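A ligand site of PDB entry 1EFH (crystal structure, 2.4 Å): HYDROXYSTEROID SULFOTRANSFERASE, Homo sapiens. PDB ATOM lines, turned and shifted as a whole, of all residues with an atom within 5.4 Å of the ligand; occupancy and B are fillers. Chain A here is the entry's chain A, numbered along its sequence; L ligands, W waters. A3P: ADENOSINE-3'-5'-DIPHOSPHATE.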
ATOM      1  N   THR A  41     -22.177 -35.831  19.654  1.00  0.00           N
ATOM      2  CA  THR A  41     -21.607 -35.715  20.983  1.00  0.00           C
ATOM      3  C   THR A  41     -22.058 -36.842  21.875  1.00  0.00           C
ATOM      4  O   THR A  41     -23.102 -37.460  21.644  1.00  0.00           O
ATOM      5  CB  THR A  41     -22.028 -34.402  21.693  1.00  0.00           C
ATOM      6  OG1 THR A  41     -23.463 -34.337  21.763  1.00  0.00           O
ATOM      7  CG2 THR A  41     -21.531 -33.188  20.967  1.00  0.00           C
ATOM      8  N   TYR A  42     -21.254 -37.139  22.883  1.00  0.00           N
ATOM      9  CA  TYR A  42     -21.633 -38.106  23.894  1.00  0.00           C
ATOM     10  C   TYR A  42     -22.424 -37.160  24.804  1.00  0.00           C
ATOM     11  O   TYR A  42     -22.023 -36.019  25.014  1.00  0.00           O
ATOM     12  CB  TYR A  42     -20.408 -38.627  24.620  1.00  0.00           C
ATOM     13  CG  TYR A  42     -20.740 -39.610  25.716  1.00  0.00           C
ATOM     14  CD1 TYR A  42     -21.014 -40.944  25.426  1.00  0.00           C
ATOM     15  CD2 TYR A  42     -20.789 -39.200  27.052  1.00  0.00           C
ATOM     16  CE1 TYR A  42     -21.315 -41.844  26.431  1.00  0.00           C
ATOM     17  CE2 TYR A  42     -21.096 -40.090  28.066  1.00  0.00           C
ATOM     18  CZ  TYR A  42     -21.356 -41.416  27.751  1.00  0.00           C
ATOM     19  OH  TYR A  42     -21.639 -42.306  28.744  1.00  0.00           O
ATOM     20  N   PRO A  43     -23.556 -37.602  25.348  1.00  0.00           N
ATOM     21  CA  PRO A  43     -24.357 -36.727  26.215  1.00  0.00           C
ATOM     22  C   PRO A  43     -23.561 -35.919  27.256  1.00  0.00           C
ATOM     23  O   PRO A  43     -22.632 -36.452  27.896  1.00  0.00           O
ATOM     24  CB  PRO A  43     -25.336 -37.691  26.876  1.00  0.00           C
ATOM     25  CG  PRO A  43     -25.506 -38.750  25.853  1.00  0.00           C
ATOM     26  CD  PRO A  43     -24.098 -38.972  25.367  1.00  0.00           C
ATOM     27  N   LYS A  44     -23.950 -34.658  27.414  1.00  0.00           N
ATOM     28  CA  LYS A  44     -23.361 -33.723  28.357  1.00  0.00           C
ATOM     29  C   LYS A  44     -21.965 -33.216  27.981  1.00  0.00           C
ATOM     30  O   LYS A  44     -21.169 -32.869  28.844  1.00  0.00           O
ATOM     31  CB  LYS A  44     -23.320 -34.351  29.765  1.00  0.00           C
ATOM     32  CG  LYS A  44     -24.585 -35.096  30.165  1.00  0.00           C
ATOM     33  CD  LYS A  44     -25.859 -34.301  29.857  1.00  0.00           C
ATOM     34  CE  LYS A  44     -25.946 -32.988  30.621  1.00  0.00           C
ATOM     35  NZ  LYS A  44     -27.046 -32.137  30.108  1.00  0.00           N
ATOM     36  N   SER A  45     -21.670 -33.170  26.679  1.00  0.00           N
ATOM     37  CA  SER A  45     -20.371 -32.687  26.220  1.00  0.00           C
ATOM     38  C   SER A  45     -20.439 -31.258  25.680  1.00  0.00           C
ATOM     39  O   SER A  45     -19.423 -30.709  25.255  1.00  0.00           O
ATOM     40  CB  SER A  45     -19.825 -33.595  25.116  1.00  0.00           C
ATOM     41  OG  SER A  45     -19.650 -34.920  25.578  1.00  0.00           O
ATOM     42  N   GLY A  46     -21.627 -30.658  25.699  1.00  0.00           N
ATOM     43  CA  GLY A  46     -21.775 -29.292  25.205  1.00  0.00           C
ATOM     44  C   GLY A  46     -22.560 -29.215  23.911  1.00  0.00           C
ATOM     45  O   GLY A  46     -22.373 -28.288  23.109  1.00  0.00           O
ATOM     46  N   THR A  47     -23.466 -30.172  23.711  1.00  0.00           N
ATOM     47  CA  THR A  47     -24.282 -30.237  22.507  1.00  0.00           C
ATOM     48  C   THR A  47     -25.073 -28.953  22.277  1.00  0.00           C
ATOM     49  O   THR A  47     -24.969 -28.327  21.219  1.00  0.00           O
ATOM     50  CB  THR A  47     -25.283 -31.406  22.583  1.00  0.00           C
ATOM     51  OG1 THR A  47     -24.638 -32.551  23.173  1.00  0.00           O
ATOM     52  CG2 THR A  47     -25.763 -31.780  21.192  1.00  0.00           C
ATOM     53  N   ASN A  48     -25.876 -28.551  23.269  1.00  0.00           N
ATOM     54  CA  ASN A  48     -26.689 -27.352  23.151  1.00  0.00           C
ATOM     55  C   ASN A  48     -25.885 -26.076  22.937  1.00  0.00           C
ATOM     56  O   ASN A  48     -26.314 -25.168  22.233  1.00  0.00           O
ATOM     57  CB  ASN A  48     -27.563 -27.206  24.394  1.00  0.00           C
ATOM     58  CG  ASN A  48     -28.675 -28.237  24.410  1.00  0.00           C
ATOM     59  OD1 ASN A  48     -29.576 -28.202  23.571  1.00  0.00           O
ATOM     60  ND2 ASN A  48     -28.603 -29.161  25.366  1.00  0.00           N
ATOM     61  N   TRP A  49     -24.697 -26.021  23.532  1.00  0.00           N
ATOM     62  CA  TRP A  49     -23.846 -24.852  23.393  1.00  0.00           C
ATOM     63  C   TRP A  49     -23.450 -24.718  21.931  1.00  0.00           C
ATOM     64  O   TRP A  49     -23.541 -23.653  21.346  1.00  0.00           O
ATOM     65  CB  TRP A  49     -22.615 -25.000  24.275  1.00  0.00           C
ATOM     66  CG  TRP A  49     -21.710 -23.805  24.297  1.00  0.00           C
ATOM     67  CD1 TRP A  49     -22.019 -22.533  23.905  1.00  0.00           C
ATOM     68  CD2 TRP A  49     -20.376 -23.751  24.821  1.00  0.00           C
ATOM     69  NE1 TRP A  49     -20.958 -21.690  24.153  1.00  0.00           N
ATOM     70  CE2 TRP A  49     -19.935 -22.413  24.713  1.00  0.00           C
ATOM     71  CE3 TRP A  49     -19.504 -24.703  25.365  1.00  0.00           C
ATOM     72  CZ2 TRP A  49     -18.665 -21.992  25.138  1.00  0.00           C
ATOM     73  CZ3 TRP A  49     -18.234 -24.295  25.794  1.00  0.00           C
ATOM     74  CH2 TRP A  49     -17.831 -22.945  25.670  1.00  0.00           C
ATOM     75  N   HIS A  99     -26.642 -38.341  19.617  1.00  0.00           N
ATOM     76  CA  HIS A  99     -25.748 -38.826  20.658  1.00  0.00           C
ATOM     77  C   HIS A  99     -25.391 -40.278  20.360  1.00  0.00           C
ATOM     78  O   HIS A  99     -24.668 -40.927  21.114  1.00  0.00           O
ATOM     79  CB  HIS A  99     -26.400 -38.729  22.045  1.00  0.00           C
ATOM     80  CG  HIS A  99     -26.643 -37.317  22.490  1.00  0.00           C
ATOM     81  ND1 HIS A  99     -25.631 -36.374  22.585  1.00  0.00           N
ATOM     82  CD2 HIS A  99     -27.781 -36.676  22.854  1.00  0.00           C
ATOM     83  CE1 HIS A  99     -26.141 -35.226  22.968  1.00  0.00           C
ATOM     84  NE2 HIS A  99     -27.449 -35.377  23.141  1.00  0.00           N
ATOM     85  N   ARG A 121     -15.503 -33.930  25.231  1.00  0.00           N
ATOM     86  CA  ARG A 121     -15.278 -33.230  26.482  1.00  0.00           C
ATOM     87  C   ARG A 121     -14.550 -34.155  27.438  1.00  0.00           C
ATOM     88  O   ARG A 121     -14.677 -35.382  27.332  1.00  0.00           O
ATOM     89  CB  ARG A 121     -16.620 -32.805  27.080  1.00  0.00           C
ATOM     90  CG  ARG A 121     -16.521 -31.878  28.274  1.00  0.00           C
ATOM     91  CD  ARG A 121     -17.892 -31.500  28.801  1.00  0.00           C
ATOM     92  NE  ARG A 121     -17.789 -30.390  29.754  1.00  0.00           N
ATOM     93  CZ  ARG A 121     -18.755 -30.006  30.588  1.00  0.00           C
ATOM     94  NH1 ARG A 121     -19.914 -30.643  30.605  1.00  0.00           N
ATOM     95  NH2 ARG A 121     -18.550 -28.990  31.410  1.00  0.00           N
ATOM     96  N   ASP A 125     -15.492 -34.357  33.462  1.00  0.00           N
ATOM     97  CA  ASP A 125     -16.452 -33.251  33.504  1.00  0.00           C
ATOM     98  C   ASP A 125     -17.798 -33.704  32.946  1.00  0.00           C
ATOM     99  O   ASP A 125     -18.852 -33.242  33.401  1.00  0.00           O
ATOM    100  CB  ASP A 125     -15.938 -32.021  32.734  1.00  0.00           C
ATOM    101  CG  ASP A 125     -14.915 -31.207  33.532  1.00  0.00           C
ATOM    102  OD1 ASP A 125     -14.910 -31.303  34.780  1.00  0.00           O
ATOM    103  OD2 ASP A 125     -14.114 -30.468  32.917  1.00  0.00           O
ATOM    104  N   SER A 129     -21.325 -33.532  34.884  1.00  0.00           N
ATOM    105  CA  SER A 129     -22.448 -32.873  34.227  1.00  0.00           C
ATOM    106  C   SER A 129     -23.673 -33.792  34.143  1.00  0.00           C
ATOM    107  O   SER A 129     -24.797 -33.370  34.408  1.00  0.00           O
ATOM    108  CB  SER A 129     -22.049 -32.398  32.826  1.00  0.00           C
ATOM    109  OG  SER A 129     -23.101 -31.664  32.221  1.00  0.00           O
ATOM    110  N   TYR A 184     -14.728 -29.429  24.067  1.00  0.00           N
ATOM    111  CA  TYR A 184     -15.432 -28.449  24.885  1.00  0.00           C
ATOM    112  C   TYR A 184     -14.371 -27.501  25.463  1.00  0.00           C
ATOM    113  O   TYR A 184     -14.580 -26.274  25.566  1.00  0.00           O
ATOM    114  CB  TYR A 184     -16.153 -29.181  26.024  1.00  0.00           C
ATOM    115  CG  TYR A 184     -16.825 -28.271  27.020  1.00  0.00           C
ATOM    116  CD1 TYR A 184     -18.195 -28.033  26.960  1.00  0.00           C
ATOM    117  CD2 TYR A 184     -16.089 -27.665  28.035  1.00  0.00           C
ATOM    118  CE1 TYR A 184     -18.824 -27.218  27.894  1.00  0.00           C
ATOM    119  CE2 TYR A 184     -16.701 -26.834  28.974  1.00  0.00           C
ATOM    120  CZ  TYR A 184     -18.074 -26.623  28.896  1.00  0.00           C
ATOM    121  OH  TYR A 184     -18.694 -25.823  29.830  1.00  0.00           O
ATOM    122  N   LYS A 188     -14.163 -23.392  25.215  1.00  0.00           N
ATOM    123  CA  LYS A 188     -14.206 -22.546  26.401  1.00  0.00           C
ATOM    124  C   LYS A 188     -12.961 -21.650  26.466  1.00  0.00           C
ATOM    125  O   LYS A 188     -13.072 -20.466  26.756  1.00  0.00           O
ATOM    126  CB  LYS A 188     -14.261 -23.425  27.676  1.00  0.00           C
ATOM    127  CG  LYS A 188     -15.363 -23.062  28.663  1.00  0.00           C
ATOM    128  CD  LYS A 188     -15.291 -21.595  29.068  1.00  0.00           C
ATOM    129  CE  LYS A 188     -16.493 -21.159  29.925  1.00  0.00           C
ATOM    130  NZ  LYS A 188     -16.474 -21.758  31.296  1.00  0.00           N
ATOM    131  N   SER A 218     -23.903 -16.420  22.819  1.00  0.00           N
ATOM    132  CA  SER A 218     -23.723 -17.849  23.063  1.00  0.00           C
ATOM    133  C   SER A 218     -23.001 -18.052  24.394  1.00  0.00           C
ATOM    134  O   SER A 218     -22.605 -19.167  24.737  1.00  0.00           O
ATOM    135  CB  SER A 218     -22.919 -18.504  21.931  1.00  0.00           C
ATOM    136  OG  SER A 218     -21.588 -18.024  21.892  1.00  0.00           O
ATOM    137  N   SER A 219     -22.832 -16.949  25.124  1.00  0.00           N
ATOM    138  CA  SER A 219     -22.169 -17.006  26.409  1.00  0.00           C
ATOM    139  C   SER A 219     -23.029 -17.814  27.368  1.00  0.00           C
ATOM    140  O   SER A 219     -24.235 -17.944  27.163  1.00  0.00           O
ATOM    141  CB  SER A 219     -21.972 -15.586  26.966  1.00  0.00           C
ATOM    142  OG  SER A 219     -23.205 -15.009  27.368  1.00  0.00           O
ATOM    143  N   PHE A 220     -22.420 -18.352  28.417  1.00  0.00           N
ATOM    144  CA  PHE A 220     -23.161 -19.144  29.387  1.00  0.00           C
ATOM    145  C   PHE A 220     -24.359 -18.367  29.933  1.00  0.00           C
ATOM    146  O   PHE A 220     -25.495 -18.848  29.859  1.00  0.00           O
ATOM    147  CB  PHE A 220     -22.245 -19.554  30.544  1.00  0.00           C
ATOM    148  CG  PHE A 220     -22.918 -20.447  31.537  1.00  0.00           C
ATOM    149  CD1 PHE A 220     -23.174 -21.784  31.238  1.00  0.00           C
ATOM    150  CD2 PHE A 220     -23.328 -19.938  32.769  1.00  0.00           C
ATOM    151  CE1 PHE A 220     -23.844 -22.603  32.155  1.00  0.00           C
ATOM    152  CE2 PHE A 220     -23.994 -20.749  33.690  1.00  0.00           C
ATOM    153  CZ  PHE A 220     -24.256 -22.089  33.379  1.00  0.00           C
ATOM    154  N   MET A 223     -27.224 -17.604  27.318  1.00  0.00           N
ATOM    155  CA  MET A 223     -28.025 -18.785  26.999  1.00  0.00           C
ATOM    156  C   MET A 223     -28.905 -19.202  28.172  1.00  0.00           C
ATOM    157  O   MET A 223     -30.043 -19.642  27.976  1.00  0.00           O
ATOM    158  CB  MET A 223     -27.133 -19.959  26.612  1.00  0.00           C
ATOM    159  CG  MET A 223     -26.606 -19.894  25.199  1.00  0.00           C
ATOM    160  SD  MET A 223     -25.720 -21.392  24.813  1.00  0.00           S
ATOM    161  CE  MET A 223     -27.042 -22.563  24.692  1.00  0.00           C
ATOM    162  N   LEU A 245     -30.512 -27.315  32.706  1.00  0.00           N
ATOM    163  CA  LEU A 245     -29.673 -27.625  31.554  1.00  0.00           C
ATOM    164  C   LEU A 245     -28.314 -26.916  31.632  1.00  0.00           C
ATOM    165  O   LEU A 245     -27.285 -27.538  31.389  1.00  0.00           O
ATOM    166  CB  LEU A 245     -30.385 -27.261  30.251  1.00  0.00           C
ATOM    167  CG  LEU A 245     -29.701 -27.650  28.935  1.00  0.00           C
ATOM    168  CD1 LEU A 245     -29.264 -29.104  28.969  1.00  0.00           C
ATOM    169  CD2 LEU A 245     -30.654 -27.396  27.761  1.00  0.00           C
ATOM    170  N   LEU A 246     -28.297 -25.626  31.938  1.00  0.00           N
ATOM    171  CA  LEU A 246     -27.029 -24.914  32.060  1.00  0.00           C
ATOM    172  C   LEU A 246     -26.737 -24.823  33.548  1.00  0.00           C
ATOM    173  O   LEU A 246     -27.369 -24.065  34.272  1.00  0.00           O
ATOM    174  CB  LEU A 246     -27.109 -23.491  31.470  1.00  0.00           C
ATOM    175  CG  LEU A 246     -27.608 -23.267  30.032  1.00  0.00           C
ATOM    176  CD1 LEU A 246     -26.760 -22.190  29.376  1.00  0.00           C
ATOM    177  CD2 LEU A 246     -27.539 -24.543  29.212  1.00  0.00           C
ATOM    178  N   ARG A 247     -25.770 -25.632  33.995  1.00  0.00           N
ATOM    179  CA  ARG A 247     -25.390 -25.703  35.399  1.00  0.00           C
ATOM    180  C   ARG A 247     -24.325 -24.678  35.802  1.00  0.00           C
ATOM    181  O   ARG A 247     -24.628 -23.693  36.470  1.00  0.00           O
ATOM    182  CB  ARG A 247     -24.911 -27.113  35.708  1.00  0.00           C
ATOM    183  CG  ARG A 247     -24.748 -27.429  37.181  1.00  0.00           C
ATOM    184  CD  ARG A 247     -24.433 -28.898  37.343  1.00  0.00           C
ATOM    185  NE  ARG A 247     -23.223 -29.267  36.627  1.00  0.00           N
ATOM    186  CZ  ARG A 247     -21.990 -29.094  37.099  1.00  0.00           C
ATOM    187  NH1 ARG A 247     -21.808 -28.554  38.298  1.00  0.00           N
ATOM    188  NH2 ARG A 247     -20.941 -29.443  36.361  1.00  0.00           N
ATOM    189  N   LYS A 248     -23.063 -24.933  35.428  1.00  0.00           N
ATOM    190  CA  LYS A 248     -21.952 -24.020  35.732  1.00  0.00           C
ATOM    191  C   LYS A 248     -21.332 -23.515  34.440  1.00  0.00           C
ATOM    192  O   LYS A 248     -20.932 -22.356  34.340  1.00  0.00           O
ATOM    193  CB  LYS A 248     -20.855 -24.714  36.546  1.00  0.00           C
ATOM    194  CG  LYS A 248     -21.188 -24.998  37.990  1.00  0.00           C
ATOM    195  CD  LYS A 248     -19.929 -25.358  38.773  1.00  0.00           C
ATOM    196  CE  LYS A 248     -18.906 -24.218  38.733  1.00  0.00           C
ATOM    197  NZ  LYS A 248     -17.738 -24.459  39.637  1.00  0.00           N
ATOM    198  N   GLY A 249     -21.240 -24.404  33.457  1.00  0.00           N
ATOM    199  CA  GLY A 249     -20.670 -24.030  32.182  1.00  0.00           C
ATOM    200  C   GLY A 249     -19.171 -23.795  32.177  1.00  0.00           C
ATOM    201  O   GLY A 249     -18.679 -23.052  31.342  1.00  0.00           O
ATOM    202  N   VAL A 250     -18.450 -24.402  33.107  1.00  0.00           N
ATOM    203  CA  VAL A 250     -17.003 -24.220  33.109  1.00  0.00           C
ATOM    204  C   VAL A 250     -16.335 -25.534  32.777  1.00  0.00           C
ATOM    205  O   VAL A 250     -16.979 -26.493  32.368  1.00  0.00           O
ATOM    206  CB  VAL A 250     -16.472 -23.728  34.486  1.00  0.00           C
ATOM    207  CG1 VAL A 250     -17.150 -22.414  34.871  1.00  0.00           C
ATOM    208  CG2 VAL A 250     -16.701 -24.799  35.554  1.00  0.00           C
HETATM  209  P1  A3P L   1     -22.112 -28.513  33.088  1.00  0.00           P
HETATM  210  O1P A3P L   1     -23.090 -29.443  33.660  1.00  0.00           O
HETATM  211  O2P A3P L   1     -22.393 -27.134  33.512  1.00  0.00           O
HETATM  212  O3P A3P L   1     -20.729 -28.892  33.436  1.00  0.00           O
HETATM  213  P2  A3P L   1     -25.083 -31.025  26.531  1.00  0.00           P
HETATM  214  O4P A3P L   1     -26.176 -31.685  27.278  1.00  0.00           O
HETATM  215  O5P A3P L   1     -25.602 -29.882  25.725  1.00  0.00           O
HETATM  216  O6P A3P L   1     -24.372 -32.001  25.676  1.00  0.00           O
HETATM  217  O5' A3P L   1     -24.031 -30.429  27.586  1.00  0.00           O
HETATM  218  C5' A3P L   1     -24.439 -29.630  28.698  1.00  0.00           C
HETATM  219  C4' A3P L   1     -23.213 -28.981  29.324  1.00  0.00           C
HETATM  220  O4' A3P L   1     -22.827 -27.824  28.497  1.00  0.00           O
HETATM  221  C3' A3P L   1     -23.425 -28.430  30.730  1.00  0.00           C
HETATM  222  O3' A3P L   1     -22.217 -28.588  31.489  1.00  0.00           O
HETATM  223  C2' A3P L   1     -23.800 -26.991  30.419  1.00  0.00           C
HETATM  224  O2' A3P L   1     -23.730 -26.050  31.470  1.00  0.00           O
HETATM  225  C1' A3P L   1     -22.790 -26.688  29.315  1.00  0.00           C
HETATM  226  N9  A3P L   1     -23.118 -25.485  28.587  1.00  0.00           N
HETATM  227  C8  A3P L   1     -24.288 -25.133  27.956  1.00  0.00           C
HETATM  228  N7  A3P L   1     -24.269 -23.945  27.390  1.00  0.00           N
HETATM  229  C5  A3P L   1     -22.997 -23.474  27.674  1.00  0.00           C
HETATM  230  C6  A3P L   1     -22.314 -22.268  27.366  1.00  0.00           C
HETATM  231  N6  A3P L   1     -22.873 -21.266  26.680  1.00  0.00           N
HETATM  232  N1  A3P L   1     -21.023 -22.129  27.810  1.00  0.00           N
HETATM  233  C2  A3P L   1     -20.437 -23.137  28.509  1.00  0.00           C
HETATM  234  N3  A3P L   1     -20.972 -24.306  28.856  1.00  0.00           N
HETATM  235  C4  A3P L   1     -22.259 -24.423  28.413  1.00  0.00           C
HETATM  236  O   HOH W   1     -19.189 -26.868  34.750  1.00  0.00           O
HETATM  237  O   HOH W   2     -24.252 -27.659  25.931  1.00  0.00           O
HETATM  238  O   HOH W   3     -25.410 -30.520  34.379  1.00  0.00           O
HETATM  239  O   HOH W   4     -18.731 -30.544  34.411  1.00  0.00           O
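The indole nitrogen (NE1) of Trp 49 sits close to a nitrogen (N6) of the ligand (3.2 Å).
The backbone NH (N) of Phe 220 lies close to a nitrogen (N6) of the ligand (3.4 Å).
Residues that only touch the ligand: Ser 219, Leu 246 and Leu 245.
Water W3 lies within hydrogen-bond range of an oxygen (O1P) of the ligand, the backbone carbonyl oxygen of Ser 129 and the guanidinium group of Arg 247.
Water W4 lies within hydrogen-bond range of an oxygen (O3P) of the ligand, the backbone carbonyl oxygen (O) of Asp 125, the guanidinium group (NH2) of Arg 247 and the guanidinium group (NH2) of Arg 121.
Water W1 lies within hydrogen-bond range of an oxygen (O3P) of the ligand (2.9 Å), the backbone NH (N) of Val 250 (3.1 Å) and the backbone NH (N) of Gly 249 (3.5 Å).
The backbone carbonyl oxygen of Ser 218 lies within hydrogen-bond range of the indole nitrogen of Trp 49 (3.1 Å).
OG1 of Thr 47 is in hydrogen-bond range of OG1 of Thr 41 (2.6 Å).
The guanidinium group (NH2) of Arg 121 sits at hydrogen-bond distance from the backbone carbonyl oxygen (O) of Val 250, at 3.1 Å.
The backbone carbonyl oxygen (O) of Gly 249 is in hydrogen-bond range of the side-chain amino group (NZ) of Lys 188.
The guanidinium group (NH1) of Arg 121 is in hydrogen-bond range of the backbone carbonyl oxygen (O) of Lys 44 (3.1 Å).
OH of Tyr 184 is in hydrogen-bond range of O of Val 250.
The side-chain hydroxyl (OG) of Ser 45 is in hydrogen-bond range of the backbone carbonyl oxygen (O) of Tyr 42, 2.7 Å away.
The side-chain hydroxyl (OH) of Tyr 184 lies close to the backbone carbonyl oxygen (O) of Gly 249, 3.2 Å away.
A nitrogen (N6) of the ligand lies within hydrogen-bond range of the side-chain sulfur of Met 223 (3.4 Å).
An oxygen (O2P) of the ligand is in hydrogen-bond range of the backbone NH (N) of Gly 249 (3.0 Å).
The side-chain hydroxyl (OG1) of Thr 47 is in hydrogen-bond range of an oxygen (O6P) of the ligand (2.6 Å).
An oxygen (O5P) of the ligand lies within hydrogen-bond range of the side-chain amide nitrogen (ND2) of Asn 48.
An oxygen (O6P) of the ligand is in hydrogen-bond range of the backbone NH (N) of Gly 46 (3.1 Å).
The guanidinium group (NE) of Arg 247 is in salt-bridge range of an oxygen (O1P) of the ligand (3.0 Å).
The backbone NH (N) of Ser 45 is in hydrogen-bond range of an oxygen (O6P) of the ligand (3.1 Å).
An oxygen (O6P) of the ligand lies within hydrogen-bond range of the backbone NH of Lys 44 (3.2 Å).
O5P of the ligand lies within hydrogen-bond range of N of Asn 48, 2.8 Å away.
O3P of the ligand lies within salt-bridge range of NH2 of Arg 121, 3.0 Å away.
A nitrogen (N3) of the ligand lies within hydrogen-bond range of the side-chain hydroxyl (OH) of Tyr 184 (2.9 Å).
The backbone NH of Lys 248 lies within hydrogen-bond range of an oxygen (O2P) of the ligand (3.0 Å).
The backbone NH (N) of Arg 247 lies within hydrogen-bond range of an oxygen (O2') of the ligand, at 3.3 Å.
The backbone carbonyl oxygen (O) of Ser 218 lies within hydrogen-bond range of a nitrogen (N6) of the ligand, at 2.9 Å.
The side-chain hydroxyl of Ser 129 sits at hydrogen-bond distance from an oxygen (O1P) of the ligand (2.6 Å).
N of Thr 47 lies within hydrogen-bond range of O6P of the ligand (2.8 Å).
O4P of the ligand is in salt-bridge range of NZ of Lys 44, at 3.0 Å.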
